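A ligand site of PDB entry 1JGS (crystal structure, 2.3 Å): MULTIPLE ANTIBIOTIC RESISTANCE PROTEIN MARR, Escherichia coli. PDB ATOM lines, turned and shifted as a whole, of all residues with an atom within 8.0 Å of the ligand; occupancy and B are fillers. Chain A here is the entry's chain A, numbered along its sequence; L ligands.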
ATOM      1  N   THR A  50     -21.457  10.302  14.865  1.00  0.00           N
ATOM      2  CA  THR A  50     -21.726  10.276  13.428  1.00  0.00           C
ATOM      3  C   THR A  50     -22.139   8.864  13.008  1.00  0.00           C
ATOM      4  O   THR A  50     -21.748   7.871  13.633  1.00  0.00           O
ATOM      5  CB  THR A  50     -20.491  10.700  12.623  1.00  0.00           C
ATOM      6  OG1 THR A  50     -19.437   9.754  12.835  1.00  0.00           O
ATOM      7  CG2 THR A  50     -20.036  12.082  13.049  1.00  0.00           C
ATOM      8  N   PRO A  51     -22.951   8.745  11.949  1.00  0.00           N
ATOM      9  CA  PRO A  51     -23.339   7.392  11.551  1.00  0.00           C
ATOM     10  C   PRO A  51     -22.119   6.538  11.204  1.00  0.00           C
ATOM     11  O   PRO A  51     -22.046   5.367  11.592  1.00  0.00           O
ATOM     12  CB  PRO A  51     -24.252   7.653  10.365  1.00  0.00           C
ATOM     13  CG  PRO A  51     -24.921   8.941  10.745  1.00  0.00           C
ATOM     14  CD  PRO A  51     -23.756   9.763  11.250  1.00  0.00           C
ATOM     15  N   VAL A  52     -21.155   7.127  10.499  1.00  0.00           N
ATOM     16  CA  VAL A  52     -19.955   6.393  10.124  1.00  0.00           C
ATOM     17  C   VAL A  52     -19.155   5.949  11.349  1.00  0.00           C
ATOM     18  O   VAL A  52     -18.673   4.817  11.398  1.00  0.00           O
ATOM     19  CB  VAL A  52     -19.062   7.217   9.203  1.00  0.00           C
ATOM     20  CG1 VAL A  52     -17.830   6.408   8.832  1.00  0.00           C
ATOM     21  CG2 VAL A  52     -19.832   7.641   7.957  1.00  0.00           C
ATOM     22  N   GLU A  53     -18.992   6.845  12.324  1.00  0.00           N
ATOM     23  CA  GLU A  53     -18.270   6.491  13.547  1.00  0.00           C
ATOM     24  C   GLU A  53     -19.060   5.368  14.220  1.00  0.00           C
ATOM     25  O   GLU A  53     -18.496   4.400  14.732  1.00  0.00           O
ATOM     26  CB  GLU A  53     -18.185   7.702  14.477  1.00  0.00           C
ATOM     27  CG  GLU A  53     -17.411   7.454  15.775  1.00  0.00           C
ATOM     28  CD  GLU A  53     -15.904   7.478  15.579  1.00  0.00           C
ATOM     29  OE1 GLU A  53     -15.380   6.643  14.808  1.00  0.00           O
ATOM     30  OE2 GLU A  53     -15.241   8.332  16.202  1.00  0.00           O
ATOM     31  N   LYS A  55     -20.911   3.307  12.729  1.00  0.00           N
ATOM     32  CA  LYS A  55     -20.722   2.161  11.852  1.00  0.00           C
ATOM     33  C   LYS A  55     -19.469   1.391  12.272  1.00  0.00           C
ATOM     34  O   LYS A  55     -19.451   0.161  12.293  1.00  0.00           O
ATOM     35  CB  LYS A  55     -20.591   2.651  10.394  1.00  0.00           C
ATOM     36  CG  LYS A  55     -20.412   1.546   9.364  1.00  0.00           C
ATOM     37  CD  LYS A  55     -19.340   1.915   8.357  1.00  0.00           C
ATOM     38  CE  LYS A  55     -18.999   0.735   7.423  1.00  0.00           C
ATOM     39  NZ  LYS A  55     -18.530  -0.507   8.142  1.00  0.00           N
ATOM     40  N   ASP A  61     -22.595  -3.436   8.486  1.00  0.00           N
ATOM     41  CA  ASP A  61     -22.728  -2.973   7.123  1.00  0.00           C
ATOM     42  C   ASP A  61     -23.364  -1.586   7.202  1.00  0.00           C
ATOM     43  O   ASP A  61     -24.342  -1.383   7.940  1.00  0.00           O
ATOM     44  CB  ASP A  61     -23.628  -3.911   6.320  1.00  0.00           C
ATOM     45  CG  ASP A  61     -23.919  -3.397   4.919  1.00  0.00           C
ATOM     46  OD1 ASP A  61     -24.923  -3.834   4.324  1.00  0.00           O
ATOM     47  OD2 ASP A  61     -23.147  -2.565   4.412  1.00  0.00           O
ATOM     48  N   LEU A  62     -22.828  -0.636   6.451  1.00  0.00           N
ATOM     49  CA  LEU A  62     -23.356   0.714   6.468  1.00  0.00           C
ATOM     50  C   LEU A  62     -24.808   0.700   6.008  1.00  0.00           C
ATOM     51  O   LEU A  62     -25.655   1.384   6.578  1.00  0.00           O
ATOM     52  CB  LEU A  62     -22.539   1.633   5.558  1.00  0.00           C
ATOM     53  CG  LEU A  62     -22.880   3.114   5.679  1.00  0.00           C
ATOM     54  CD1 LEU A  62     -22.572   3.572   7.086  1.00  0.00           C
ATOM     55  CD2 LEU A  62     -22.082   3.941   4.675  1.00  0.00           C
ATOM     56  N   GLY A  63     -25.094  -0.089   4.977  1.00  0.00           N
ATOM     57  CA  GLY A  63     -26.444  -0.160   4.451  1.00  0.00           C
ATOM     58  C   GLY A  63     -27.479  -0.531   5.499  1.00  0.00           C
ATOM     59  O   GLY A  63     -28.563   0.056   5.560  1.00  0.00           O
ATOM     60  N   ALA A  64     -27.151  -1.509   6.331  1.00  0.00           N
ATOM     61  CA  ALA A  64     -28.069  -1.978   7.359  1.00  0.00           C
ATOM     62  C   ALA A  64     -28.189  -0.964   8.491  1.00  0.00           C
ATOM     63  O   ALA A  64     -29.191  -0.950   9.205  1.00  0.00           O
ATOM     64  CB  ALA A  64     -27.603  -3.312   7.906  1.00  0.00           C
ATOM     65  N   LEU A  65     -27.172  -0.129   8.639  1.00  0.00           N
ATOM     66  CA  LEU A  65     -27.166   0.880   9.691  1.00  0.00           C
ATOM     67  C   LEU A  65     -28.121   2.009   9.307  1.00  0.00           C
ATOM     68  O   LEU A  65     -28.933   2.472  10.126  1.00  0.00           O
ATOM     69  CB  LEU A  65     -25.758   1.450   9.880  1.00  0.00           C
ATOM     70  CG  LEU A  65     -25.641   2.417  11.063  1.00  0.00           C
ATOM     71  CD1 LEU A  65     -25.866   1.631  12.338  1.00  0.00           C
ATOM     72  CD2 LEU A  65     -24.281   3.091  11.069  1.00  0.00           C
ATOM     73  N   THR A  66     -28.032   2.431   8.051  1.00  0.00           N
ATOM     74  CA  THR A  66     -28.851   3.484   7.498  1.00  0.00           C
ATOM     75  C   THR A  66     -30.316   3.149   7.640  1.00  0.00           C
ATOM     76  O   THR A  66     -31.112   3.977   8.091  1.00  0.00           O
ATOM     77  CB  THR A  66     -28.554   3.698   5.991  1.00  0.00           C
ATOM     78  OG1 THR A  66     -27.145   3.740   5.776  1.00  0.00           O
ATOM     79  CG2 THR A  66     -29.176   4.990   5.498  1.00  0.00           C
ATOM     80  N   ARG A  67     -30.683   1.928   7.247  1.00  0.00           N
ATOM     81  CA  ARG A  67     -32.078   1.495   7.357  1.00  0.00           C
ATOM     82  C   ARG A  67     -32.416   1.440   8.837  1.00  0.00           C
ATOM     83  O   ARG A  67     -33.494   1.829   9.238  1.00  0.00           O
ATOM     84  CB  ARG A  67     -32.280   0.114   6.717  1.00  0.00           C
ATOM     85  CG  ARG A  67     -31.995   0.060   5.220  1.00  0.00           C
ATOM     86  CD  ARG A  67     -32.697  -1.118   4.552  1.00  0.00           C
ATOM     87  NE  ARG A  67     -32.321  -2.416   5.118  1.00  0.00           N
ATOM     88  CZ  ARG A  67     -31.151  -3.012   4.923  1.00  0.00           C
ATOM     89  NH1 ARG A  67     -30.218  -2.433   4.182  1.00  0.00           N
ATOM     90  NH2 ARG A  67     -30.915  -4.186   5.492  1.00  0.00           N
ATOM     91  N   MET A  68     -31.470   0.948   9.622  1.00  0.00           N
ATOM     92  CA  MET A  68     -31.644   0.850  11.071  1.00  0.00           C
ATOM     93  C   MET A  68     -31.908   2.229  11.686  1.00  0.00           C
ATOM     94  O   MET A  68     -32.841   2.415  12.479  1.00  0.00           O
ATOM     95  CB  MET A  68     -30.382   0.250  11.710  1.00  0.00           C
ATOM     96  CG  MET A  68     -30.293   0.423  13.212  1.00  0.00           C
ATOM     97  SD  MET A  68     -31.526  -0.541  14.082  1.00  0.00           S
ATOM     98  CE  MET A  68     -30.571  -2.084  14.335  1.00  0.00           C
ATOM     99  N   LEU A  69     -31.072   3.206  11.320  1.00  0.00           N
ATOM    100  CA  LEU A  69     -31.239   4.539  11.864  1.00  0.00           C
ATOM    101  C   LEU A  69     -32.602   5.116  11.456  1.00  0.00           C
ATOM    102  O   LEU A  69     -33.278   5.761  12.270  1.00  0.00           O
ATOM    103  CB  LEU A  69     -30.082   5.435  11.418  1.00  0.00           C
ATOM    104  CG  LEU A  69     -28.717   5.125  12.074  1.00  0.00           C
ATOM    105  CD1 LEU A  69     -27.637   6.016  11.464  1.00  0.00           C
ATOM    106  CD2 LEU A  69     -28.777   5.410  13.579  1.00  0.00           C
ATOM    107  N   ASP A  70     -33.018   4.845  10.224  1.00  0.00           N
ATOM    108  CA  ASP A  70     -34.318   5.348   9.750  1.00  0.00           C
ATOM    109  C   ASP A  70     -35.429   4.675  10.534  1.00  0.00           C
ATOM    110  O   ASP A  70     -36.398   5.326  10.915  1.00  0.00           O
ATOM    111  CB  ASP A  70     -34.513   5.085   8.250  1.00  0.00           C
ATOM    112  CG  ASP A  70     -33.884   6.177   7.371  1.00  0.00           C
ATOM    113  OD1 ASP A  70     -33.403   7.208   7.886  1.00  0.00           O
ATOM    114  OD2 ASP A  70     -33.900   5.989   6.132  1.00  0.00           O
ATOM    115  N   VAL A  73     -35.682   6.327  13.866  1.00  0.00           N
ATOM    116  CA  VAL A  73     -36.282   7.662  13.817  1.00  0.00           C
ATOM    117  C   VAL A  73     -37.802   7.483  13.730  1.00  0.00           C
ATOM    118  O   VAL A  73     -38.541   8.189  14.410  1.00  0.00           O
ATOM    119  CB  VAL A  73     -35.781   8.467  12.600  1.00  0.00           C
ATOM    120  CG1 VAL A  73     -36.542   9.773  12.473  1.00  0.00           C
ATOM    121  CG2 VAL A  73     -34.280   8.732  12.762  1.00  0.00           C
ATOM    122  N   ARG A  80     -31.582  13.226  14.190  1.00  0.00           N
ATOM    123  CA  ARG A  80     -30.390  13.690  13.511  1.00  0.00           C
ATOM    124  C   ARG A  80     -30.176  15.200  13.618  1.00  0.00           C
ATOM    125  O   ARG A  80     -31.113  15.984  13.433  1.00  0.00           O
ATOM    126  CB  ARG A  80     -30.493  13.319  12.035  1.00  0.00           C
ATOM    127  CG  ARG A  80     -29.301  12.583  11.478  1.00  0.00           C
ATOM    128  CD  ARG A  80     -29.634  12.151  10.080  1.00  0.00           C
ATOM    129  NE  ARG A  80     -30.864  11.393  10.101  1.00  0.00           N
ATOM    130  CZ  ARG A  80     -30.958  10.087   9.833  1.00  0.00           C
ATOM    131  NH1 ARG A  80     -29.876   9.405   9.506  1.00  0.00           N
ATOM    132  NH2 ARG A  80     -32.134   9.477   9.907  1.00  0.00           N
ATOM    133  N   ARG A  88     -20.981  18.869   6.189  1.00  0.00           N
ATOM    134  CA  ARG A  88     -21.438  18.012   5.116  1.00  0.00           C
ATOM    135  C   ARG A  88     -21.990  16.751   5.771  1.00  0.00           C
ATOM    136  O   ARG A  88     -22.360  15.791   5.095  1.00  0.00           O
ATOM    137  CB  ARG A  88     -20.263  17.656   4.200  1.00  0.00           C
ATOM    138  CG  ARG A  88     -20.645  16.914   2.928  1.00  0.00           C
ATOM    139  CD  ARG A  88     -21.242  17.859   1.891  1.00  0.00           C
ATOM    140  NE  ARG A  88     -20.215  18.693   1.272  1.00  0.00           N
ATOM    141  CZ  ARG A  88     -19.313  18.239   0.406  1.00  0.00           C
ATOM    142  NH1 ARG A  88     -19.307  16.962   0.069  1.00  0.00           N
ATOM    143  NH2 ARG A  88     -18.394  19.071  -0.085  1.00  0.00           N
ATOM    144  N   GLY A  89     -22.037  16.752   7.097  1.00  0.00           N
ATOM    145  CA  GLY A  89     -22.508  15.596   7.812  1.00  0.00           C
ATOM    146  C   GLY A  89     -23.450  15.869   8.964  1.00  0.00           C
ATOM    147  O   GLY A  89     -23.781  17.021   9.271  1.00  0.00           O
ATOM    148  N   VAL A  90     -23.889  14.797   9.616  1.00  0.00           N
ATOM    149  CA  VAL A  90     -24.801  14.915  10.732  1.00  0.00           C
ATOM    150  C   VAL A  90     -24.399  14.012  11.871  1.00  0.00           C
ATOM    151  O   VAL A  90     -23.508  13.167  11.718  1.00  0.00           O
ATOM    152  CB  VAL A  90     -26.251  14.533  10.343  1.00  0.00           C
ATOM    153  CG1 VAL A  90     -26.751  15.458   9.256  1.00  0.00           C
ATOM    154  CG2 VAL A  90     -26.325  13.085   9.898  1.00  0.00           C
ATOM    155  N   LEU A  91     -25.052  14.197  13.002  1.00  0.00           N
ATOM    156  CA  LEU A  91     -24.796  13.394  14.172  1.00  0.00           C
ATOM    157  C   LEU A  91     -26.156  12.803  14.486  1.00  0.00           C
ATOM    158  O   LEU A  91     -27.178  13.311  14.029  1.00  0.00           O
ATOM    159  CB  LEU A  91     -24.344  14.265  15.368  1.00  0.00           C
ATOM    160  CG  LEU A  91     -23.005  15.025  15.346  1.00  0.00           C
ATOM    161  CD1 LEU A  91     -23.054  16.116  16.395  1.00  0.00           C
ATOM    162  CD2 LEU A  91     -21.815  14.101  15.621  1.00  0.00           C
ATOM    163  N   VAL A  92     -26.166  11.736  15.250  1.00  0.00           N
ATOM    164  CA  VAL A  92     -27.425  11.148  15.635  1.00  0.00           C
ATOM    165  C   VAL A  92     -27.328  11.040  17.133  1.00  0.00           C
ATOM    166  O   VAL A  92     -26.272  10.727  17.682  1.00  0.00           O
ATOM    167  CB  VAL A  92     -27.647   9.754  15.021  1.00  0.00           C
ATOM    168  CG1 VAL A  92     -27.748   9.859  13.477  1.00  0.00           C
ATOM    169  CG2 VAL A  92     -26.510   8.825  15.422  1.00  0.00           C
HETATM  170  C1  LIG L   1     -27.267   8.674   7.713  1.00  0.00           C
HETATM  171  O1  LIG L   1     -27.645   9.949   7.821  1.00  0.00           O
HETATM  172  O2  LIG L   1     -28.053   7.764   7.989  1.00  0.00           O
HETATM  173  C2  LIG L   1     -25.884   8.429   7.265  1.00  0.00           C
HETATM  174  C3  LIG L   1     -25.388   7.075   7.122  1.00  0.00           C
HETATM  175  C4  LIG L   1     -24.065   6.809   6.705  1.00  0.00           C
HETATM  176  C5  LIG L   1     -23.191   7.850   6.403  1.00  0.00           C
HETATM  177  C6  LIG L   1     -23.705   9.339   6.535  1.00  0.00           C
HETATM  178  C7  LIG L   1     -25.006   9.536   6.963  1.00  0.00           C
HETATM  179  O3  LIG L   1     -26.160   5.982   7.394  1.00  0.00           O
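OG1 of Thr 66 lies within hydrogen-bond range of O3 of the ligand, 2.9 Å away. An oxygen (O1) of the ligand lies within salt-bridge range of the guanidinium group of Arg 80 (2.8 Å).
NH2 of Arg 80 lies within salt-bridge range of OD1 of Asp 70, 3.3 Å away. The side-chain hydroxyl (OG1) of Thr 66 lies within hydrogen-bond range of the backbone carbonyl oxygen (O) of Leu 62, 2.9 Å away.
Merely in contact with the ligand: Pro 51 (3.5 Å), Val 52 (3.7 Å), Leu 62 (3.6 Å), Leu 69 (3.9 Å) and Val 90 (3.99 Å). Hydrophobic or aromatic side chains that line the ligand: Pro 51, Val 52, Leu 62, Leu 69 and Val 90. Within 4 Å of the ligand: Pro 51, Val 52, Leu 62, Thr 66, Leu 69, Arg 80 and Val 90. The nearest printed residue that does not touch the ligand is Leu 65 (4.8 Å).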
